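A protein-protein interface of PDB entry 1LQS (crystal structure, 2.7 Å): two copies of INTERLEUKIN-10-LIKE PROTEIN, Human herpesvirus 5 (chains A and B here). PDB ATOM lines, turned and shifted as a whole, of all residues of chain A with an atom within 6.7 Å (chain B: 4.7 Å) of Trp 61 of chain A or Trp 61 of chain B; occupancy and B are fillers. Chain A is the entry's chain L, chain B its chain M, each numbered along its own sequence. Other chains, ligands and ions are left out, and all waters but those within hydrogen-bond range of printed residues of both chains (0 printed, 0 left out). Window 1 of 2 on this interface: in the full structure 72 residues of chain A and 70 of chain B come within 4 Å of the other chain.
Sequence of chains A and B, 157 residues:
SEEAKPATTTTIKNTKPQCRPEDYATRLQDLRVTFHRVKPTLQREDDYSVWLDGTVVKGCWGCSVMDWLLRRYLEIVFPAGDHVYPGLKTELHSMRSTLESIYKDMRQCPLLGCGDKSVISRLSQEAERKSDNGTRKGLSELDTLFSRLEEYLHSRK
Of the 11 printed residues of chain B, 10 touch a printed residue of chain A.
Printed residues of chain B that touch a printed residue of chain A: Cys 60, Trp 61, Gly 62, Cys 63, Ser 64, Val 65, Cys 114, Gly 115, Asp 116 and Arg 156.
Hydrophobic or aromatic side chains of chain B that line the printed part of chain A: Trp 61 and Val 65.
Printed residues of chain A that touch a printed residue of chain B: Cys 60, Trp 61, Cys 63, Ser 64, Gly 113, Cys 114, Gly 115, Asp 116, Val 119 and Tyr 152.
Along chain A the printed residues that touch a printed residue of chain B span positions 60 to 152.
SG of Cys 63 of chain B forms a disulfide with SG of Cys 114 of chain B, 2.0 Å away.
N of Ser 64 of chain B sits at hydrogen-bond distance from SG of Cys 114 of chain B.
The backbone NH (N) of Ser 64 of chain A is in hydrogen-bond range of the side-chain sulfur (SG) of Cys 114 of chain A.
SG of Cys 63 of chain A is disulfide-bonded to SG of Cys 114 of chain A (2.0 Å).
Of the printed residues of chain B, Cys 60 of chain A touches Cys 60 and Trp 61.
Printed residues of chain B within 4 Å of Trp 61 of chain A: Cys 60 (3.6 Å), Trp 61 (3.9 Å), Cys 63 (3.2 Å), Cys 114 (3.4 Å), Gly 115 (3.3 Å) and Asp 116 (3.2 Å).
Of the printed residues of chain B, Cys 63 of chain A touches Trp 61 and Arg 156.
Gly 59 of chain B touches none of the printed residues of chain A.
Trp 61 of chain B touches just these residues of chain A: Cys 60 (3.7 Å), Trp 61 (3.9 Å), Cys 63 (3.6 Å), Cys 114 (3.9 Å), Gly 115 (3.1 Å) and Asp 116 (3.3 Å).
Of the printed residues of chain A, Cys 63 of chain B touches Trp 61 (3.2 Å) and Tyr 152 (3.1 Å).
The nearest printed residue of chain B that does not touch Trp 61 of chain A is Ser 64 of chain B (4.01 Å).
The nearest residue of chain A that does not touch Trp 61 of chain B is Gly 113 of chain A (4.8 Å).
Trp 61 of chain A touches Cys 114 of chain B, and with the chains exchanged Cys 114 of chain A touches Trp 61 of chain B.
Trp 61 of chain A touches Gly 115 of chain B, and with the chains exchanged Gly 115 of chain A touches Trp 61 of chain B.
Trp 61 of chain A touches Asp 116 of chain B, and with the chains exchanged Asp 116 of chain A touches Trp 61 of chain B.
Cys 63 of chain A touches Arg 156 of chain B, but with the chains exchanged Arg 156 of chain A does not touch Cys 63 of chain B (4.1 Å).
Positions printed for both chains: 59, 60, 61, 62, 63, 64, 65, 114, 115, 116 and 156.
Of the 19 pairs that touch across the chains among the printed residues, 14 have their exchanged pair printed and touching as well.
Among the printed residues, merely in contact across the chains: Cys 63 of chain A with Arg 156 of chain B, Tyr 152 of chain A with Cys 63 of chain B, Gly 115 of chain A with Trp 61 of chain B, Trp 61 of chain A with Asp 116 of chain B, Asp 116 of chain A with Trp 61 of chain B, Trp 61 of chain A with Gly 115 of chain B, Trp 61 of chain A with Cys 114 of chain B, Trp 61 of chain A with Cys 60 of chain B, Cys 63 of chain A with Trp 61 of chain B, Cys 60 of chain A with Trp 61 of chain B, Tyr 152 of chain A with Gly 62 of chain B, Trp 61 of chain A with Trp 61 of chain B, Val 119 of chain A with Val 65 of chain B, Cys 114 of chain A with Trp 61 of chain B and Gly 113 of chain A with Arg 156 of chain B.
The side-chain sulfur (SG) of Cys 60 of chain B is disulfide-bonded to the side-chain sulfur (SG) of Cys 60 of chain A (2.0 Å).
The indole nitrogen (NE1) of Trp 61 of chain A lies close to the side-chain sulfur (SG) of Cys 63 of chain B (3.6 Å).
The side-chain hydroxyl (OG) of Ser 64 of chain A is in hydrogen-bond range of the side-chain carboxylate (OD2) of Asp 116 of chain B (3.2 Å).
The side-chain carboxylate (OD2) of Asp 116 of chain A sits at hydrogen-bond distance from the side-chain hydroxyl (OG) of Ser 64 of chain B, 2.6 Å away.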
ATOM      1  N   VAL A  56      25.036 -25.841   6.974  1.00  0.00           N
ATOM      2  CA  VAL A  56      23.704 -25.674   6.424  1.00  0.00           C
ATOM      3  C   VAL A  56      22.566 -25.850   7.415  1.00  0.00           C
ATOM      4  O   VAL A  56      21.593 -25.090   7.404  1.00  0.00           O
ATOM      5  CB  VAL A  56      23.501 -26.665   5.257  1.00  0.00           C
ATOM      6  CG1 VAL A  56      23.264 -28.062   5.800  1.00  0.00           C
ATOM      7  CG2 VAL A  56      22.355 -26.213   4.363  1.00  0.00           C
ATOM      8  N   VAL A  57      22.689 -26.851   8.277  1.00  0.00           N
ATOM      9  CA  VAL A  57      21.646 -27.151   9.241  1.00  0.00           C
ATOM     10  C   VAL A  57      22.086 -26.929  10.697  1.00  0.00           C
ATOM     11  O   VAL A  57      21.376 -27.275  11.643  1.00  0.00           O
ATOM     12  CB  VAL A  57      21.118 -28.602   8.950  1.00  0.00           C
ATOM     13  CG1 VAL A  57      21.045 -29.445  10.209  1.00  0.00           C
ATOM     14  CG2 VAL A  57      19.752 -28.515   8.270  1.00  0.00           C
ATOM     15  N   LYS A  58      23.260 -26.323  10.854  1.00  0.00           N
ATOM     16  CA  LYS A  58      23.833 -25.990  12.165  1.00  0.00           C
ATOM     17  C   LYS A  58      23.563 -24.523  12.497  1.00  0.00           C
ATOM     18  O   LYS A  58      23.017 -23.773  11.682  1.00  0.00           O
ATOM     19  CB  LYS A  58      25.353 -26.218  12.187  1.00  0.00           C
ATOM     20  CG  LYS A  58      25.766 -27.676  12.188  1.00  0.00           C
ATOM     21  CD  LYS A  58      27.264 -27.848  12.359  1.00  0.00           C
ATOM     22  CE  LYS A  58      27.643 -29.316  12.281  1.00  0.00           C
ATOM     23  NZ  LYS A  58      29.114 -29.508  12.264  1.00  0.00           N
ATOM     24  N   GLY A  59      23.959 -24.105  13.690  1.00  0.00           N
ATOM     25  CA  GLY A  59      23.721 -22.727  14.072  1.00  0.00           C
ATOM     26  C   GLY A  59      22.319 -22.589  14.633  1.00  0.00           C
ATOM     27  O   GLY A  59      21.496 -23.493  14.464  1.00  0.00           O
ATOM     28  N   CYS A  60      22.053 -21.461  15.291  1.00  0.00           N
ATOM     29  CA  CYS A  60      20.758 -21.175  15.909  1.00  0.00           C
ATOM     30  C   CYS A  60      19.538 -21.523  15.072  1.00  0.00           C
ATOM     31  O   CYS A  60      18.583 -22.118  15.579  1.00  0.00           O
ATOM     32  CB  CYS A  60      20.650 -19.691  16.272  1.00  0.00           C
ATOM     33  SG  CYS A  60      21.110 -19.179  17.961  1.00  0.00           S
ATOM     34  N   TRP A  61      19.550 -21.158  13.794  1.00  0.00           N
ATOM     35  CA  TRP A  61      18.372 -21.427  12.991  1.00  0.00           C
ATOM     36  C   TRP A  61      18.356 -22.649  12.096  1.00  0.00           C
ATOM     37  O   TRP A  61      17.505 -22.757  11.210  1.00  0.00           O
ATOM     38  CB  TRP A  61      17.985 -20.170  12.208  1.00  0.00           C
ATOM     39  CG  TRP A  61      17.384 -19.129  13.120  1.00  0.00           C
ATOM     40  CD1 TRP A  61      18.020 -18.049  13.672  1.00  0.00           C
ATOM     41  CD2 TRP A  61      16.056 -19.141  13.681  1.00  0.00           C
ATOM     42  NE1 TRP A  61      17.171 -17.395  14.543  1.00  0.00           N
ATOM     43  CE2 TRP A  61      15.964 -18.044  14.567  1.00  0.00           C
ATOM     44  CE3 TRP A  61      14.939 -19.975  13.524  1.00  0.00           C
ATOM     45  CZ2 TRP A  61      14.801 -17.761  15.292  1.00  0.00           C
ATOM     46  CZ3 TRP A  61      13.784 -19.689  14.249  1.00  0.00           C
ATOM     47  CH2 TRP A  61      13.727 -18.591  15.121  1.00  0.00           C
ATOM     48  N   GLY A  62      19.271 -23.584  12.351  1.00  0.00           N
ATOM     49  CA  GLY A  62      19.317 -24.804  11.566  1.00  0.00           C
ATOM     50  C   GLY A  62      17.956 -25.481  11.538  1.00  0.00           C
ATOM     51  O   GLY A  62      17.532 -25.992  10.505  1.00  0.00           O
ATOM     52  N   CYS A  63      17.272 -25.483  12.679  1.00  0.00           N
ATOM     53  CA  CYS A  63      15.947 -26.074  12.786  1.00  0.00           C
ATOM     54  C   CYS A  63      15.094 -25.567  11.626  1.00  0.00           C
ATOM     55  O   CYS A  63      14.349 -26.310  11.000  1.00  0.00           O
ATOM     56  CB  CYS A  63      15.299 -25.667  14.124  1.00  0.00           C
ATOM     57  SG  CYS A  63      15.111 -23.862  14.362  1.00  0.00           S
ATOM     58  N   SER A  64      15.224 -24.282  11.344  1.00  0.00           N
ATOM     59  CA  SER A  64      14.473 -23.653  10.277  1.00  0.00           C
ATOM     60  C   SER A  64      14.919 -24.189   8.925  1.00  0.00           C
ATOM     61  O   SER A  64      14.102 -24.448   8.040  1.00  0.00           O
ATOM     62  CB  SER A  64      14.688 -22.138  10.348  1.00  0.00           C
ATOM     63  OG  SER A  64      13.846 -21.434   9.462  1.00  0.00           O
ATOM     64  N   VAL A  65      16.223 -24.357   8.759  1.00  0.00           N
ATOM     65  CA  VAL A  65      16.742 -24.851   7.487  1.00  0.00           C
ATOM     66  C   VAL A  65      16.434 -26.332   7.310  1.00  0.00           C
ATOM     67  O   VAL A  65      16.199 -26.790   6.200  1.00  0.00           O
ATOM     68  CB  VAL A  65      18.276 -24.633   7.375  1.00  0.00           C
ATOM     69  CG1 VAL A  65      18.799 -25.269   6.105  1.00  0.00           C
ATOM     70  CG2 VAL A  65      18.597 -23.139   7.389  1.00  0.00           C
ATOM     71  N   MET A  66      16.422 -27.071   8.413  1.00  0.00           N
ATOM     72  CA  MET A  66      16.154 -28.499   8.363  1.00  0.00           C
ATOM     73  C   MET A  66      14.759 -28.748   7.827  1.00  0.00           C
ATOM     74  O   MET A  66      14.563 -29.670   7.026  1.00  0.00           O
ATOM     75  CB  MET A  66      16.296 -29.134   9.754  1.00  0.00           C
ATOM     76  CG  MET A  66      16.307 -30.671   9.767  1.00  0.00           C
ATOM     77  SD  MET A  66      17.843 -31.435   9.129  1.00  0.00           S
ATOM     78  CE  MET A  66      17.390 -31.620   7.434  1.00  0.00           C
ATOM     79  N   GLY A 113      12.021 -29.358  16.436  1.00  0.00           N
ATOM     80  CA  GLY A 113      11.756 -28.220  15.574  1.00  0.00           C
ATOM     81  C   GLY A 113      12.394 -26.981  16.170  1.00  0.00           C
ATOM     82  O   GLY A 113      13.342 -27.086  16.954  1.00  0.00           O
ATOM     83  N   CYS A 114      11.899 -25.803  15.813  1.00  0.00           N
ATOM     84  CA  CYS A 114      12.479 -24.596  16.376  1.00  0.00           C
ATOM     85  C   CYS A 114      11.851 -24.315  17.726  1.00  0.00           C
ATOM     86  O   CYS A 114      10.692 -24.657  17.963  1.00  0.00           O
ATOM     87  CB  CYS A 114      12.280 -23.403  15.456  1.00  0.00           C
ATOM     88  SG  CYS A 114      13.174 -23.480  13.874  1.00  0.00           S
ATOM     89  N   GLY A 115      12.628 -23.688  18.604  1.00  0.00           N
ATOM     90  CA  GLY A 115      12.166 -23.391  19.943  1.00  0.00           C
ATOM     91  C   GLY A 115      11.218 -22.228  20.099  1.00  0.00           C
ATOM     92  O   GLY A 115      10.359 -22.242  20.973  1.00  0.00           O
ATOM     93  N   ASP A 116      11.358 -21.218  19.259  1.00  0.00           N
ATOM     94  CA  ASP A 116      10.484 -20.073  19.368  1.00  0.00           C
ATOM     95  C   ASP A 116       9.027 -20.515  19.401  1.00  0.00           C
ATOM     96  O   ASP A 116       8.256 -20.047  20.238  1.00  0.00           O
ATOM     97  CB  ASP A 116      10.723 -19.104  18.208  1.00  0.00           C
ATOM     98  CG  ASP A 116      10.043 -19.538  16.939  1.00  0.00           C
ATOM     99  OD1 ASP A 116      10.389 -20.627  16.418  1.00  0.00           O
ATOM    100  OD2 ASP A 116       9.155 -18.788  16.472  1.00  0.00           O
ATOM    101  N   LYS A 117       8.652 -21.431  18.513  1.00  0.00           N
ATOM    102  CA  LYS A 117       7.268 -21.911  18.458  1.00  0.00           C
ATOM    103  C   LYS A 117       6.717 -22.318  19.823  1.00  0.00           C
ATOM    104  O   LYS A 117       5.516 -22.237  20.057  1.00  0.00           O
ATOM    105  CB  LYS A 117       7.131 -23.096  17.489  1.00  0.00           C
ATOM    106  CG  LYS A 117       7.439 -22.770  16.032  1.00  0.00           C
ATOM    107  CD  LYS A 117       7.052 -23.935  15.116  1.00  0.00           C
ATOM    108  CE  LYS A 117       7.196 -23.580  13.618  1.00  0.00           C
ATOM    109  NZ  LYS A 117       6.749 -24.691  12.701  1.00  0.00           N
ATOM    110  N   VAL A 119       7.840 -21.040  23.051  1.00  0.00           N
ATOM    111  CA  VAL A 119       7.693 -19.869  23.905  1.00  0.00           C
ATOM    112  C   VAL A 119       6.447 -19.072  23.507  1.00  0.00           C
ATOM    113  O   VAL A 119       5.626 -18.733  24.366  1.00  0.00           O
ATOM    114  CB  VAL A 119       8.933 -18.961  23.810  1.00  0.00           C
ATOM    115  CG1 VAL A 119       8.725 -17.697  24.640  1.00  0.00           C
ATOM    116  CG2 VAL A 119      10.168 -19.722  24.293  1.00  0.00           C
ATOM    117  N   TYR A 152      16.914  -6.793  24.725  1.00  0.00           N
ATOM    118  CA  TYR A 152      17.043  -7.456  23.429  1.00  0.00           C
ATOM    119  C   TYR A 152      17.952  -6.670  22.483  1.00  0.00           C
ATOM    120  O   TYR A 152      18.933  -7.210  21.978  1.00  0.00           O
ATOM    121  CB  TYR A 152      15.667  -7.645  22.775  1.00  0.00           C
ATOM    122  CG  TYR A 152      15.733  -8.269  21.402  1.00  0.00           C
ATOM    123  CD1 TYR A 152      15.913  -9.644  21.245  1.00  0.00           C
ATOM    124  CD2 TYR A 152      15.664  -7.480  20.256  1.00  0.00           C
ATOM    125  CE1 TYR A 152      16.025 -10.215  19.985  1.00  0.00           C
ATOM    126  CE2 TYR A 152      15.779  -8.042  18.997  1.00  0.00           C
ATOM    127  CZ  TYR A 152      15.961  -9.411  18.869  1.00  0.00           C
ATOM    128  OH  TYR A 152      16.100  -9.965  17.616  1.00  0.00           O
ATOM    129  N   ARG A 156      22.345  -8.374  20.556  1.00  0.00           N
ATOM    130  CA  ARG A 156      22.956  -8.674  19.270  1.00  0.00           C
ATOM    131  C   ARG A 156      23.654  -7.457  18.697  1.00  0.00           C
ATOM    132  O   ARG A 156      24.851  -7.256  19.017  1.00  0.00           O
ATOM    133  CB  ARG A 156      21.898  -9.146  18.275  1.00  0.00           C
ATOM    134  CG  ARG A 156      20.644  -8.282  18.222  1.00  0.00           C
ATOM    135  CD  ARG A 156      19.531  -8.926  19.007  1.00  0.00           C
ATOM    136  NE  ARG A 156      19.471 -10.372  18.788  1.00  0.00           N
ATOM    137  CZ  ARG A 156      19.405 -10.966  17.593  1.00  0.00           C
ATOM    138  NH1 ARG A 156      19.396 -10.251  16.476  1.00  0.00           N
ATOM    139  NH2 ARG A 156      19.322 -12.286  17.515  1.00  0.00           N
ATOM    140  N   GLY B  59      18.221 -15.991  24.154  1.00  0.00           N
ATOM    141  CA  GLY B  59      18.526 -17.151  23.336  1.00  0.00           C
ATOM    142  C   GLY B  59      18.308 -17.032  21.840  1.00  0.00           C
ATOM    143  O   GLY B  59      18.050 -15.945  21.315  1.00  0.00           O
ATOM    144  N   CYS B  60      18.426 -18.178  21.165  1.00  0.00           N
ATOM    145  CA  CYS B  60      18.262 -18.299  19.719  1.00  0.00           C
ATOM    146  C   CYS B  60      16.866 -17.852  19.270  1.00  0.00           C
ATOM    147  O   CYS B  60      16.696 -17.149  18.271  1.00  0.00           O
ATOM    148  CB  CYS B  60      18.455 -19.762  19.293  1.00  0.00           C
ATOM    149  SG  CYS B  60      20.135 -20.469  19.175  1.00  0.00           S
ATOM    150  N   TRP B  61      15.875 -18.279  20.035  1.00  0.00           N
ATOM    151  CA  TRP B  61      14.476 -17.990  19.767  1.00  0.00           C
ATOM    152  C   TRP B  61      14.079 -16.526  19.998  1.00  0.00           C
ATOM    153  O   TRP B  61      13.044 -16.074  19.495  1.00  0.00           O
ATOM    154  CB  TRP B  61      13.629 -18.907  20.655  1.00  0.00           C
ATOM    155  CG  TRP B  61      14.149 -20.323  20.664  1.00  0.00           C
ATOM    156  CD1 TRP B  61      14.279 -21.157  21.750  1.00  0.00           C
ATOM    157  CD2 TRP B  61      14.656 -21.053  19.536  1.00  0.00           C
ATOM    158  NE1 TRP B  61      14.845 -22.353  21.367  1.00  0.00           N
ATOM    159  CE2 TRP B  61      15.088 -22.321  20.017  1.00  0.00           C
ATOM    160  CE3 TRP B  61      14.794 -20.758  18.165  1.00  0.00           C
ATOM    161  CZ2 TRP B  61      15.646 -23.296  19.173  1.00  0.00           C
ATOM    162  CZ3 TRP B  61      15.349 -21.724  17.327  1.00  0.00           C
ATOM    163  CH2 TRP B  61      15.771 -22.984  17.839  1.00  0.00           C
ATOM    164  N   GLY B  62      14.902 -15.804  20.761  1.00  0.00           N
ATOM    165  CA  GLY B  62      14.631 -14.416  21.080  1.00  0.00           C
ATOM    166  C   GLY B  62      14.160 -13.513  19.955  1.00  0.00           C
ATOM    167  O   GLY B  62      13.115 -12.869  20.082  1.00  0.00           O
ATOM    168  N   CYS B  63      14.923 -13.446  18.865  1.00  0.00           N
ATOM    169  CA  CYS B  63      14.550 -12.598  17.732  1.00  0.00           C
ATOM    170  C   CYS B  63      13.076 -12.807  17.372  1.00  0.00           C
ATOM    171  O   CYS B  63      12.343 -11.848  17.134  1.00  0.00           O
ATOM    172  CB  CYS B  63      15.417 -12.920  16.494  1.00  0.00           C
ATOM    173  SG  CYS B  63      15.216 -14.643  15.929  1.00  0.00           S
ATOM    174  N   SER B  64      12.650 -14.069  17.342  1.00  0.00           N
ATOM    175  CA  SER B  64      11.282 -14.415  16.975  1.00  0.00           C
ATOM    176  C   SER B  64      10.244 -14.012  18.007  1.00  0.00           C
ATOM    177  O   SER B  64       9.203 -13.439  17.669  1.00  0.00           O
ATOM    178  CB  SER B  64      11.189 -15.916  16.705  1.00  0.00           C
ATOM    179  OG  SER B  64       9.862 -16.300  16.404  1.00  0.00           O
ATOM    180  N   VAL B  65      10.528 -14.313  19.266  1.00  0.00           N
ATOM    181  CA  VAL B  65       9.607 -13.976  20.339  1.00  0.00           C
ATOM    182  C   VAL B  65       9.408 -12.458  20.400  1.00  0.00           C
ATOM    183  O   VAL B  65       8.284 -11.985  20.495  1.00  0.00           O
ATOM    184  CB  VAL B  65      10.128 -14.521  21.696  1.00  0.00           C
ATOM    185  CG1 VAL B  65       9.100 -14.304  22.783  1.00  0.00           C
ATOM    186  CG2 VAL B  65      10.416 -16.001  21.575  1.00  0.00           C
ATOM    187  N   CYS B 114      15.579 -12.362  12.945  1.00  0.00           N
ATOM    188  CA  CYS B 114      16.065 -13.733  12.929  1.00  0.00           C
ATOM    189  C   CYS B 114      17.000 -14.077  11.777  1.00  0.00           C
ATOM    190  O   CYS B 114      16.693 -13.816  10.620  1.00  0.00           O
ATOM    191  CB  CYS B 114      14.885 -14.675  12.906  1.00  0.00           C
ATOM    192  SG  CYS B 114      13.869 -14.569  14.402  1.00  0.00           S
ATOM    193  N   GLY B 115      18.140 -14.671  12.113  1.00  0.00           N
ATOM    194  CA  GLY B 115      19.111 -15.050  11.108  1.00  0.00           C
ATOM    195  C   GLY B 115      18.815 -16.442  10.593  1.00  0.00           C
ATOM    196  O   GLY B 115      19.599 -17.373  10.800  1.00  0.00           O
ATOM    197  N   ASP B 116      17.675 -16.581   9.918  1.00  0.00           N
ATOM    198  CA  ASP B 116      17.258 -17.866   9.380  1.00  0.00           C
ATOM    199  C   ASP B 116      16.808 -17.771   7.925  1.00  0.00           C
ATOM    200  O   ASP B 116      16.533 -18.790   7.288  1.00  0.00           O
ATOM    201  CB  ASP B 116      16.123 -18.436  10.233  1.00  0.00           C
ATOM    202  CG  ASP B 116      14.861 -17.618  10.135  1.00  0.00           C
ATOM    203  OD1 ASP B 116      14.937 -16.377  10.246  1.00  0.00           O
ATOM    204  OD2 ASP B 116      13.787 -18.222   9.949  1.00  0.00           O
ATOM    205  N   ARG B 156      19.984 -31.937  18.799  1.00  0.00           N
ATOM    206  CA  ARG B 156      18.787 -31.442  19.479  1.00  0.00           C
ATOM    207  C   ARG B 156      18.594 -32.065  20.862  1.00  0.00           C
ATOM    208  O   ARG B 156      17.650 -32.872  21.019  1.00  0.00           O
ATOM    209  CB  ARG B 156      17.544 -31.702  18.617  1.00  0.00           C
ATOM    210  CG  ARG B 156      17.115 -30.509  17.777  1.00  0.00           C
ATOM    211  CD  ARG B 156      18.233 -29.985  16.868  1.00  0.00           C
ATOM    212  NE  ARG B 156      17.845 -28.741  16.199  1.00  0.00           N
ATOM    213  CZ  ARG B 156      17.569 -27.599  16.833  1.00  0.00           C
ATOM    214  NH1 ARG B 156      17.643 -27.531  18.159  1.00  0.00           N
ATOM    215  NH2 ARG B 156      17.206 -26.521  16.144  1.00  0.00           N
